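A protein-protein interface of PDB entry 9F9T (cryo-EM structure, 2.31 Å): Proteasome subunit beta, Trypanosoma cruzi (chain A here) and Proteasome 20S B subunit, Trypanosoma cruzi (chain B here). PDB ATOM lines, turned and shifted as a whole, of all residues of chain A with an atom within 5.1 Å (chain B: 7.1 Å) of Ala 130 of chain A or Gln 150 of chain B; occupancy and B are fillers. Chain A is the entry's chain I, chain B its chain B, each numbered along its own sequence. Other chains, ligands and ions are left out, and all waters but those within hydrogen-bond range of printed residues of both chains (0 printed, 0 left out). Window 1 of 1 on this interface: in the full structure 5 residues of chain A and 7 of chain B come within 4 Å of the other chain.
The side-chain carboxylate (OD1) of Asp 124 of chain B is in hydrogen-bond range of the side-chain amide nitrogen (NE2) of Gln 150 of chain B, 3.2 Å away.
Among the printed residues, pairs that only touch across the chains: Leu 134 of chain A with Leu 123 of chain B (3.4 Å), Leu 131 of chain A with Arg 146 of chain B (3.5 Å), Leu 134 of chain A with Arg 146 of chain B (3.7 Å), Leu 131 of chain A with Gln 150 of chain B (3.8 Å), Leu 131 of chain A with Lys 147 of chain B (3.8 Å), Ala 130 of chain A with Gln 150 of chain B (3.9 Å), Ala 127 of chain A with Gln 150 of chain B (3.9 Å) and Ala 127 of chain A with Leu 154 of chain B (3.9 Å).
Of the printed residues of chain B, Ala 127 of chain A touches Gln 150 and Leu 154.
Ala 130 of chain A touches one residue of chain B.
Of the printed residues of chain B, Leu 134 of chain A touches Leu 123 and Arg 146.
Printed residues of chain A within 4 Å of Arg 146 of chain B: Leu 131 (3.5 Å) and Leu 134 (3.7 Å).
Printed residues of chain A within 4 Å of Lys 147 of chain B: Leu 131.
Gln 150 of chain B touches just these residues of chain A: Ala 127, Ala 130 and Leu 131.
The nearest printed residue of chain A that does not touch Arg 146 of chain B is Arg 133 of chain A (6.7 Å).
Hydrophobic or aromatic side chains of chain B that line the printed part of chain A: Leu 154.
Hydrophobic or aromatic side chains of chain A that line the printed part of chain B: Ala 127, Ala 130, Leu 131 and Leu 134.
Among the printed residues, 8 pairs touch across the chains.
Among the printed residues, no Asp or Glu carboxylate lies within 4 Å of a Lys or Arg side-chain nitrogen of the other chain.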
ATOM      1  N   VAL A 125     -19.755  16.597  10.256  1.00  0.00           N
ATOM      2  CA  VAL A 125     -21.158  16.769  10.483  1.00  0.00           C
ATOM      3  C   VAL A 125     -21.490  16.708  11.955  1.00  0.00           C
ATOM      4  O   VAL A 125     -22.451  17.267  12.416  1.00  0.00           O
ATOM      5  CB  VAL A 125     -21.940  15.762   9.633  1.00  0.00           C
ATOM      6  CG1 VAL A 125     -23.428  15.628  10.035  1.00  0.00           C
ATOM      7  CG2 VAL A 125     -21.849  16.123   8.150  1.00  0.00           C
ATOM      8  N   SER A 126     -20.763  16.004  12.749  1.00  0.00           N
ATOM      9  CA  SER A 126     -21.055  16.071  14.170  1.00  0.00           C
ATOM     10  C   SER A 126     -20.715  17.459  14.754  1.00  0.00           C
ATOM     11  O   SER A 126     -21.492  18.002  15.543  1.00  0.00           O
ATOM     12  CB  SER A 126     -20.280  14.985  14.800  1.00  0.00           C
ATOM     13  OG  SER A 126     -20.608  14.891  16.165  1.00  0.00           O
ATOM     14  N   ALA A 127     -19.629  18.102  14.305  1.00  0.00           N
ATOM     15  CA  ALA A 127     -19.346  19.433  14.733  1.00  0.00           C
ATOM     16  C   ALA A 127     -20.421  20.398  14.272  1.00  0.00           C
ATOM     17  O   ALA A 127     -20.829  21.278  15.010  1.00  0.00           O
ATOM     18  CB  ALA A 127     -18.007  19.911  14.200  1.00  0.00           C
ATOM     19  N   ASN A 128     -20.902  20.252  13.033  1.00  0.00           N
ATOM     20  CA  ASN A 128     -21.887  21.202  12.548  1.00  0.00           C
ATOM     21  C   ASN A 128     -23.257  20.994  13.183  1.00  0.00           C
ATOM     22  O   ASN A 128     -24.021  21.953  13.310  1.00  0.00           O
ATOM     23  CB  ASN A 128     -21.986  21.193  11.040  1.00  0.00           C
ATOM     24  CG  ASN A 128     -20.768  21.792  10.368  1.00  0.00           C
ATOM     25  OD1 ASN A 128     -19.962  22.493  10.960  1.00  0.00           O
ATOM     26  ND2 ASN A 128     -20.621  21.464   9.101  1.00  0.00           N
ATOM     27  N   LEU A 129     -23.540  19.783  13.614  1.00  0.00           N
ATOM     28  CA  LEU A 129     -24.781  19.564  14.322  1.00  0.00           C
ATOM     29  C   LEU A 129     -24.755  20.188  15.684  1.00  0.00           C
ATOM     30  O   LEU A 129     -25.819  20.612  16.140  1.00  0.00           O
ATOM     31  CB  LEU A 129     -25.040  18.068  14.501  1.00  0.00           C
ATOM     32  CG  LEU A 129     -25.573  17.347  13.254  1.00  0.00           C
ATOM     33  CD1 LEU A 129     -25.580  15.868  13.520  1.00  0.00           C
ATOM     34  CD2 LEU A 129     -26.985  17.806  12.908  1.00  0.00           C
ATOM     35  N   ALA A 130     -23.578  20.159  16.343  1.00  0.00           N
ATOM     36  CA  ALA A 130     -23.387  20.785  17.670  1.00  0.00           C
ATOM     37  C   ALA A 130     -23.578  22.295  17.644  1.00  0.00           C
ATOM     38  O   ALA A 130     -24.236  22.799  18.506  1.00  0.00           O
ATOM     39  CB  ALA A 130     -22.033  20.465  18.225  1.00  0.00           C
ATOM     40  N   LEU A 131     -23.049  23.027  16.670  1.00  0.00           N
ATOM     41  CA  LEU A 131     -23.357  24.452  16.543  1.00  0.00           C
ATOM     42  C   LEU A 131     -24.815  24.671  16.342  1.00  0.00           C
ATOM     43  O   LEU A 131     -25.401  25.523  16.992  1.00  0.00           O
ATOM     44  CB  LEU A 131     -22.704  25.015  15.300  1.00  0.00           C
ATOM     45  CG  LEU A 131     -21.198  25.050  15.417  1.00  0.00           C
ATOM     46  CD1 LEU A 131     -20.595  25.287  14.065  1.00  0.00           C
ATOM     47  CD2 LEU A 131     -20.787  26.137  16.425  1.00  0.00           C
ATOM     48  N   HIS A 132     -25.407  23.910  15.439  1.00  0.00           N
ATOM     49  CA  HIS A 132     -26.836  24.001  15.239  1.00  0.00           C
ATOM     50  C   HIS A 132     -27.661  23.771  16.505  1.00  0.00           C
ATOM     51  O   HIS A 132     -28.626  24.490  16.714  1.00  0.00           O
ATOM     52  CB  HIS A 132     -27.232  23.102  14.085  1.00  0.00           C
ATOM     53  CG  HIS A 132     -28.572  23.383  13.530  1.00  0.00           C
ATOM     54  ND1 HIS A 132     -29.508  22.386  13.385  1.00  0.00           N
ATOM     55  CD2 HIS A 132     -29.118  24.498  13.031  1.00  0.00           C
ATOM     56  CE1 HIS A 132     -30.607  22.932  12.861  1.00  0.00           C
ATOM     57  NE2 HIS A 132     -30.381  24.204  12.633  1.00  0.00           N
ATOM     58  N   ARG A 133     -27.318  22.817  17.382  1.00  0.00           N
ATOM     59  CA  ARG A 133     -28.042  22.744  18.629  1.00  0.00           C
ATOM     60  C   ARG A 133     -27.776  23.949  19.544  1.00  0.00           C
ATOM     61  O   ARG A 133     -28.704  24.450  20.196  1.00  0.00           O
ATOM     62  CB  ARG A 133     -27.590  21.612  19.546  1.00  0.00           C
ATOM     63  CG  ARG A 133     -27.929  20.208  19.089  1.00  0.00           C
ATOM     64  CD  ARG A 133     -27.953  19.313  20.320  1.00  0.00           C
ATOM     65  NE  ARG A 133     -26.590  18.931  20.646  1.00  0.00           N
ATOM     66  CZ  ARG A 133     -25.795  18.319  19.804  1.00  0.00           C
ATOM     67  NH1 ARG A 133     -26.179  17.952  18.609  1.00  0.00           N
ATOM     68  NH2 ARG A 133     -24.539  18.218  20.091  1.00  0.00           N
ATOM     69  N   LEU A 134     -26.544  24.466  19.630  1.00  0.00           N
ATOM     70  CA  LEU A 134     -26.368  25.653  20.467  1.00  0.00           C
ATOM     71  C   LEU A 134     -27.195  26.815  19.948  1.00  0.00           C
ATOM     72  O   LEU A 134     -27.783  27.520  20.716  1.00  0.00           O
ATOM     73  CB  LEU A 134     -24.901  26.013  20.570  1.00  0.00           C
ATOM     74  CG  LEU A 134     -24.166  25.114  21.534  1.00  0.00           C
ATOM     75  CD1 LEU A 134     -22.684  25.384  21.526  1.00  0.00           C
ATOM     76  CD2 LEU A 134     -24.683  25.276  22.911  1.00  0.00           C
ATOM     77  N   LEU B 123     -21.276  28.138  25.370  1.00  0.00           N
ATOM     78  CA  LEU B 123     -20.400  28.245  24.222  1.00  0.00           C
ATOM     79  C   LEU B 123     -19.911  26.871  23.744  1.00  0.00           C
ATOM     80  O   LEU B 123     -19.704  26.641  22.561  1.00  0.00           O
ATOM     81  CB  LEU B 123     -19.271  29.189  24.593  1.00  0.00           C
ATOM     82  CG  LEU B 123     -19.661  30.617  24.969  1.00  0.00           C
ATOM     83  CD1 LEU B 123     -18.444  31.508  25.090  1.00  0.00           C
ATOM     84  CD2 LEU B 123     -20.563  31.270  23.975  1.00  0.00           C
ATOM     85  N   ASP B 124     -19.711  25.954  24.675  1.00  0.00           N
ATOM     86  CA  ASP B 124     -19.424  24.569  24.397  1.00  0.00           C
ATOM     87  C   ASP B 124     -19.718  23.833  25.683  1.00  0.00           C
ATOM     88  O   ASP B 124     -20.107  24.434  26.674  1.00  0.00           O
ATOM     89  CB  ASP B 124     -18.000  24.371  23.884  1.00  0.00           C
ATOM     90  CG  ASP B 124     -17.716  23.001  23.213  1.00  0.00           C
ATOM     91  OD1 ASP B 124     -18.730  22.246  22.921  1.00  0.00           O
ATOM     92  OD2 ASP B 124     -16.477  22.660  22.955  1.00  0.00           O
ATOM     93  N   ASP B 125     -19.578  22.519  25.693  1.00  0.00           N
ATOM     94  CA  ASP B 125     -19.958  21.764  26.884  1.00  0.00           C
ATOM     95  C   ASP B 125     -19.243  22.251  28.154  1.00  0.00           C
ATOM     96  O   ASP B 125     -19.830  22.187  29.239  1.00  0.00           O
ATOM     97  CB  ASP B 125     -19.932  20.261  26.552  1.00  0.00           C
ATOM     98  CG  ASP B 125     -18.595  19.547  26.441  1.00  0.00           C
ATOM     99  OD1 ASP B 125     -17.534  20.196  26.706  1.00  0.00           O
ATOM    100  OD2 ASP B 125     -18.620  18.320  26.084  1.00  0.00           O
ATOM    101  N   ALA B 145     -17.364  32.682  19.042  1.00  0.00           N
ATOM    102  CA  ALA B 145     -16.779  31.854  20.077  1.00  0.00           C
ATOM    103  C   ALA B 145     -17.156  30.369  19.960  1.00  0.00           C
ATOM    104  O   ALA B 145     -16.336  29.453  20.153  1.00  0.00           O
ATOM    105  CB  ALA B 145     -17.272  32.422  21.376  1.00  0.00           C
ATOM    106  N   ARG B 146     -18.471  30.153  19.720  1.00  0.00           N
ATOM    107  CA  ARG B 146     -19.033  28.832  19.517  1.00  0.00           C
ATOM    108  C   ARG B 146     -18.363  28.159  18.331  1.00  0.00           C
ATOM    109  O   ARG B 146     -18.019  26.987  18.451  1.00  0.00           O
ATOM    110  CB  ARG B 146     -20.517  28.909  19.226  1.00  0.00           C
ATOM    111  CG  ARG B 146     -21.353  29.098  20.463  1.00  0.00           C
ATOM    112  CD  ARG B 146     -22.784  29.381  20.139  1.00  0.00           C
ATOM    113  NE  ARG B 146     -23.497  29.287  21.391  1.00  0.00           N
ATOM    114  CZ  ARG B 146     -24.704  29.741  21.581  1.00  0.00           C
ATOM    115  NH1 ARG B 146     -25.329  30.400  20.641  1.00  0.00           N
ATOM    116  NH2 ARG B 146     -25.259  29.626  22.757  1.00  0.00           N
ATOM    117  N   LYS B 147     -18.192  28.856  17.217  1.00  0.00           N
ATOM    118  CA  LYS B 147     -17.445  28.262  16.130  1.00  0.00           C
ATOM    119  C   LYS B 147     -16.000  27.939  16.478  1.00  0.00           C
ATOM    120  O   LYS B 147     -15.520  26.881  16.060  1.00  0.00           O
ATOM    121  CB  LYS B 147     -17.311  29.125  14.889  1.00  0.00           C
ATOM    122  CG  LYS B 147     -18.615  29.425  14.188  1.00  0.00           C
ATOM    123  CD  LYS B 147     -18.373  30.074  12.835  1.00  0.00           C
ATOM    124  CE  LYS B 147     -19.230  29.459  11.747  1.00  0.00           C
ATOM    125  NZ  LYS B 147     -19.784  30.499  10.847  1.00  0.00           N
ATOM    126  N   ALA B 148     -15.305  28.808  17.212  1.00  0.00           N
ATOM    127  CA  ALA B 148     -13.892  28.546  17.417  1.00  0.00           C
ATOM    128  C   ALA B 148     -13.717  27.305  18.251  1.00  0.00           C
ATOM    129  O   ALA B 148     -12.728  26.585  18.064  1.00  0.00           O
ATOM    130  CB  ALA B 148     -13.204  29.646  18.140  1.00  0.00           C
ATOM    131  N   CYS B 149     -14.613  27.100  19.219  1.00  0.00           N
ATOM    132  CA  CYS B 149     -14.574  25.880  20.020  1.00  0.00           C
ATOM    133  C   CYS B 149     -14.756  24.621  19.195  1.00  0.00           C
ATOM    134  O   CYS B 149     -14.036  23.657  19.411  1.00  0.00           O
ATOM    135  CB  CYS B 149     -15.705  25.836  21.023  1.00  0.00           C
ATOM    136  SG  CYS B 149     -15.494  26.977  22.411  1.00  0.00           S
ATOM    137  N   GLN B 150     -15.720  24.599  18.263  1.00  0.00           N
ATOM    138  CA  GLN B 150     -15.890  23.383  17.468  1.00  0.00           C
ATOM    139  C   GLN B 150     -14.660  23.167  16.587  1.00  0.00           C
ATOM    140  O   GLN B 150     -14.136  22.062  16.502  1.00  0.00           O
ATOM    141  CB  GLN B 150     -17.172  23.379  16.645  1.00  0.00           C
ATOM    142  CG  GLN B 150     -18.405  23.409  17.513  1.00  0.00           C
ATOM    143  CD  GLN B 150     -18.436  22.228  18.455  1.00  0.00           C
ATOM    144  OE1 GLN B 150     -18.225  21.065  18.083  1.00  0.00           O
ATOM    145  NE2 GLN B 150     -18.742  22.544  19.710  1.00  0.00           N
ATOM    146  N   LYS B 151     -14.165  24.240  16.004  1.00  0.00           N
ATOM    147  CA  LYS B 151     -12.947  24.191  15.226  1.00  0.00           C
ATOM    148  C   LYS B 151     -11.772  23.596  16.000  1.00  0.00           C
ATOM    149  O   LYS B 151     -10.987  22.841  15.426  1.00  0.00           O
ATOM    150  CB  LYS B 151     -12.621  25.558  14.611  1.00  0.00           C
ATOM    151  CG  LYS B 151     -11.246  25.559  13.977  1.00  0.00           C
ATOM    152  CD  LYS B 151     -10.860  26.790  13.163  1.00  0.00           C
ATOM    153  CE  LYS B 151      -9.493  26.597  12.504  1.00  0.00           C
ATOM    154  NZ  LYS B 151      -8.539  27.679  12.852  1.00  0.00           N
ATOM    155  N   TYR B 152     -11.647  23.898  17.277  1.00  0.00           N
ATOM    156  CA  TYR B 152     -10.525  23.395  18.050  1.00  0.00           C
ATOM    157  C   TYR B 152     -10.681  21.882  18.264  1.00  0.00           C
ATOM    158  O   TYR B 152      -9.734  21.109  18.204  1.00  0.00           O
ATOM    159  CB  TYR B 152     -10.503  24.249  19.349  1.00  0.00           C
ATOM    160  CG  TYR B 152      -9.290  23.971  20.231  1.00  0.00           C
ATOM    161  CD1 TYR B 152      -8.177  24.793  20.208  1.00  0.00           C
ATOM    162  CD2 TYR B 152      -9.257  22.880  21.085  1.00  0.00           C
ATOM    163  CE1 TYR B 152      -7.058  24.532  20.978  1.00  0.00           C
ATOM    164  CE2 TYR B 152      -8.119  22.562  21.826  1.00  0.00           C
ATOM    165  CZ  TYR B 152      -7.001  23.399  21.764  1.00  0.00           C
ATOM    166  OH  TYR B 152      -5.892  23.149  22.530  1.00  0.00           O
ATOM    167  N   ARG B 153     -11.923  21.461  18.534  1.00  0.00           N
ATOM    168  CA  ARG B 153     -12.268  20.053  18.650  1.00  0.00           C
ATOM    169  C   ARG B 153     -11.889  19.306  17.390  1.00  0.00           C
ATOM    170  O   ARG B 153     -11.221  18.280  17.470  1.00  0.00           O
ATOM    171  CB  ARG B 153     -13.753  19.929  18.975  1.00  0.00           C
ATOM    172  CG  ARG B 153     -14.002  19.735  20.456  1.00  0.00           C
ATOM    173  CD  ARG B 153     -15.488  19.667  20.680  1.00  0.00           C
ATOM    174  NE  ARG B 153     -15.819  20.008  22.062  1.00  0.00           N
ATOM    175  CZ  ARG B 153     -15.465  19.291  23.122  1.00  0.00           C
ATOM    176  NH1 ARG B 153     -15.694  19.772  24.336  1.00  0.00           N
ATOM    177  NH2 ARG B 153     -14.834  18.141  22.950  1.00  0.00           N
ATOM    178  N   LEU B 154     -12.304  19.801  16.228  1.00  0.00           N
ATOM    179  CA  LEU B 154     -12.024  19.061  14.995  1.00  0.00           C
ATOM    180  C   LEU B 154     -10.547  18.852  14.836  1.00  0.00           C
ATOM    181  O   LEU B 154     -10.160  17.840  14.297  1.00  0.00           O
ATOM    182  CB  LEU B 154     -12.515  19.810  13.768  1.00  0.00           C
ATOM    183  CG  LEU B 154     -14.025  19.811  13.616  1.00  0.00           C
ATOM    184  CD1 LEU B 154     -14.424  20.844  12.600  1.00  0.00           C
ATOM    185  CD2 LEU B 154     -14.536  18.447  13.121  1.00  0.00           C
ATOM    186  N   THR B 155      -9.763  19.855  15.194  1.00  0.00           N
ATOM    187  CA  THR B 155      -8.332  19.779  15.064  1.00  0.00           C
ATOM    188  C   THR B 155      -7.742  18.922  16.154  1.00  0.00           C
ATOM    189  O   THR B 155      -6.905  18.122  15.788  1.00  0.00           O
ATOM    190  CB  THR B 155      -7.676  21.163  15.088  1.00  0.00           C
ATOM    191  OG1 THR B 155      -8.217  21.932  14.037  1.00  0.00           O
ATOM    192  CG2 THR B 155      -6.199  21.150  14.851  1.00  0.00           C
ATOM    193  N   TYR B 156      -8.015  19.089  17.442  1.00  0.00           N
ATOM    194  CA  TYR B 156      -7.187  18.439  18.466  1.00  0.00           C
ATOM    195  C   TYR B 156      -7.938  17.355  19.241  1.00  0.00           C
ATOM    196  O   TYR B 156      -7.365  16.737  20.133  1.00  0.00           O
ATOM    197  CB  TYR B 156      -6.643  19.465  19.458  1.00  0.00           C
ATOM    198  CG  TYR B 156      -5.787  20.576  18.848  1.00  0.00           C
ATOM    199  CD1 TYR B 156      -4.446  20.348  18.590  1.00  0.00           C
ATOM    200  CD2 TYR B 156      -6.321  21.816  18.493  1.00  0.00           C
ATOM    201  CE1 TYR B 156      -3.642  21.316  18.001  1.00  0.00           C
ATOM    202  CE2 TYR B 156      -5.519  22.811  17.960  1.00  0.00           C
ATOM    203  CZ  TYR B 156      -4.175  22.558  17.672  1.00  0.00           C
ATOM    204  OH  TYR B 156      -3.333  23.451  17.019  1.00  0.00           O
ATOM    205  N   GLU B 158     -10.167  17.623  21.508  1.00  0.00           N
ATOM    206  CA  GLU B 158     -10.348  17.913  22.909  1.00  0.00           C
ATOM    207  C   GLU B 158     -10.895  19.328  23.013  1.00  0.00           C
ATOM    208  O   GLU B 158     -10.888  20.086  22.051  1.00  0.00           O
ATOM    209  CB  GLU B 158      -9.028  17.698  23.662  1.00  0.00           C
ATOM    210  CG  GLU B 158      -8.009  18.777  23.466  1.00  0.00           C
ATOM    211  CD  GLU B 158      -6.798  18.746  24.392  1.00  0.00           C
ATOM    212  OE1 GLU B 158      -6.256  17.657  24.657  1.00  0.00           O
ATOM    213  OE2 GLU B 158      -6.364  19.866  24.807  1.00  0.00           O
ATOM    214  N   MET B 160     -11.443  23.218  23.763  1.00  0.00           N
ATOM    215  CA  MET B 160     -10.554  24.341  23.656  1.00  0.00           C
ATOM    216  C   MET B 160     -10.341  24.898  25.060  1.00  0.00           C
ATOM    217  O   MET B 160     -11.327  25.157  25.739  1.00  0.00           O
ATOM    218  CB  MET B 160     -11.214  25.442  22.825  1.00  0.00           C
ATOM    219  CG  MET B 160     -10.378  26.710  22.662  1.00  0.00           C
ATOM    220  SD  MET B 160     -11.237  27.657  21.454  1.00  0.00           S
ATOM    221  CE  MET B 160      -9.880  28.473  20.617  1.00  0.00           C
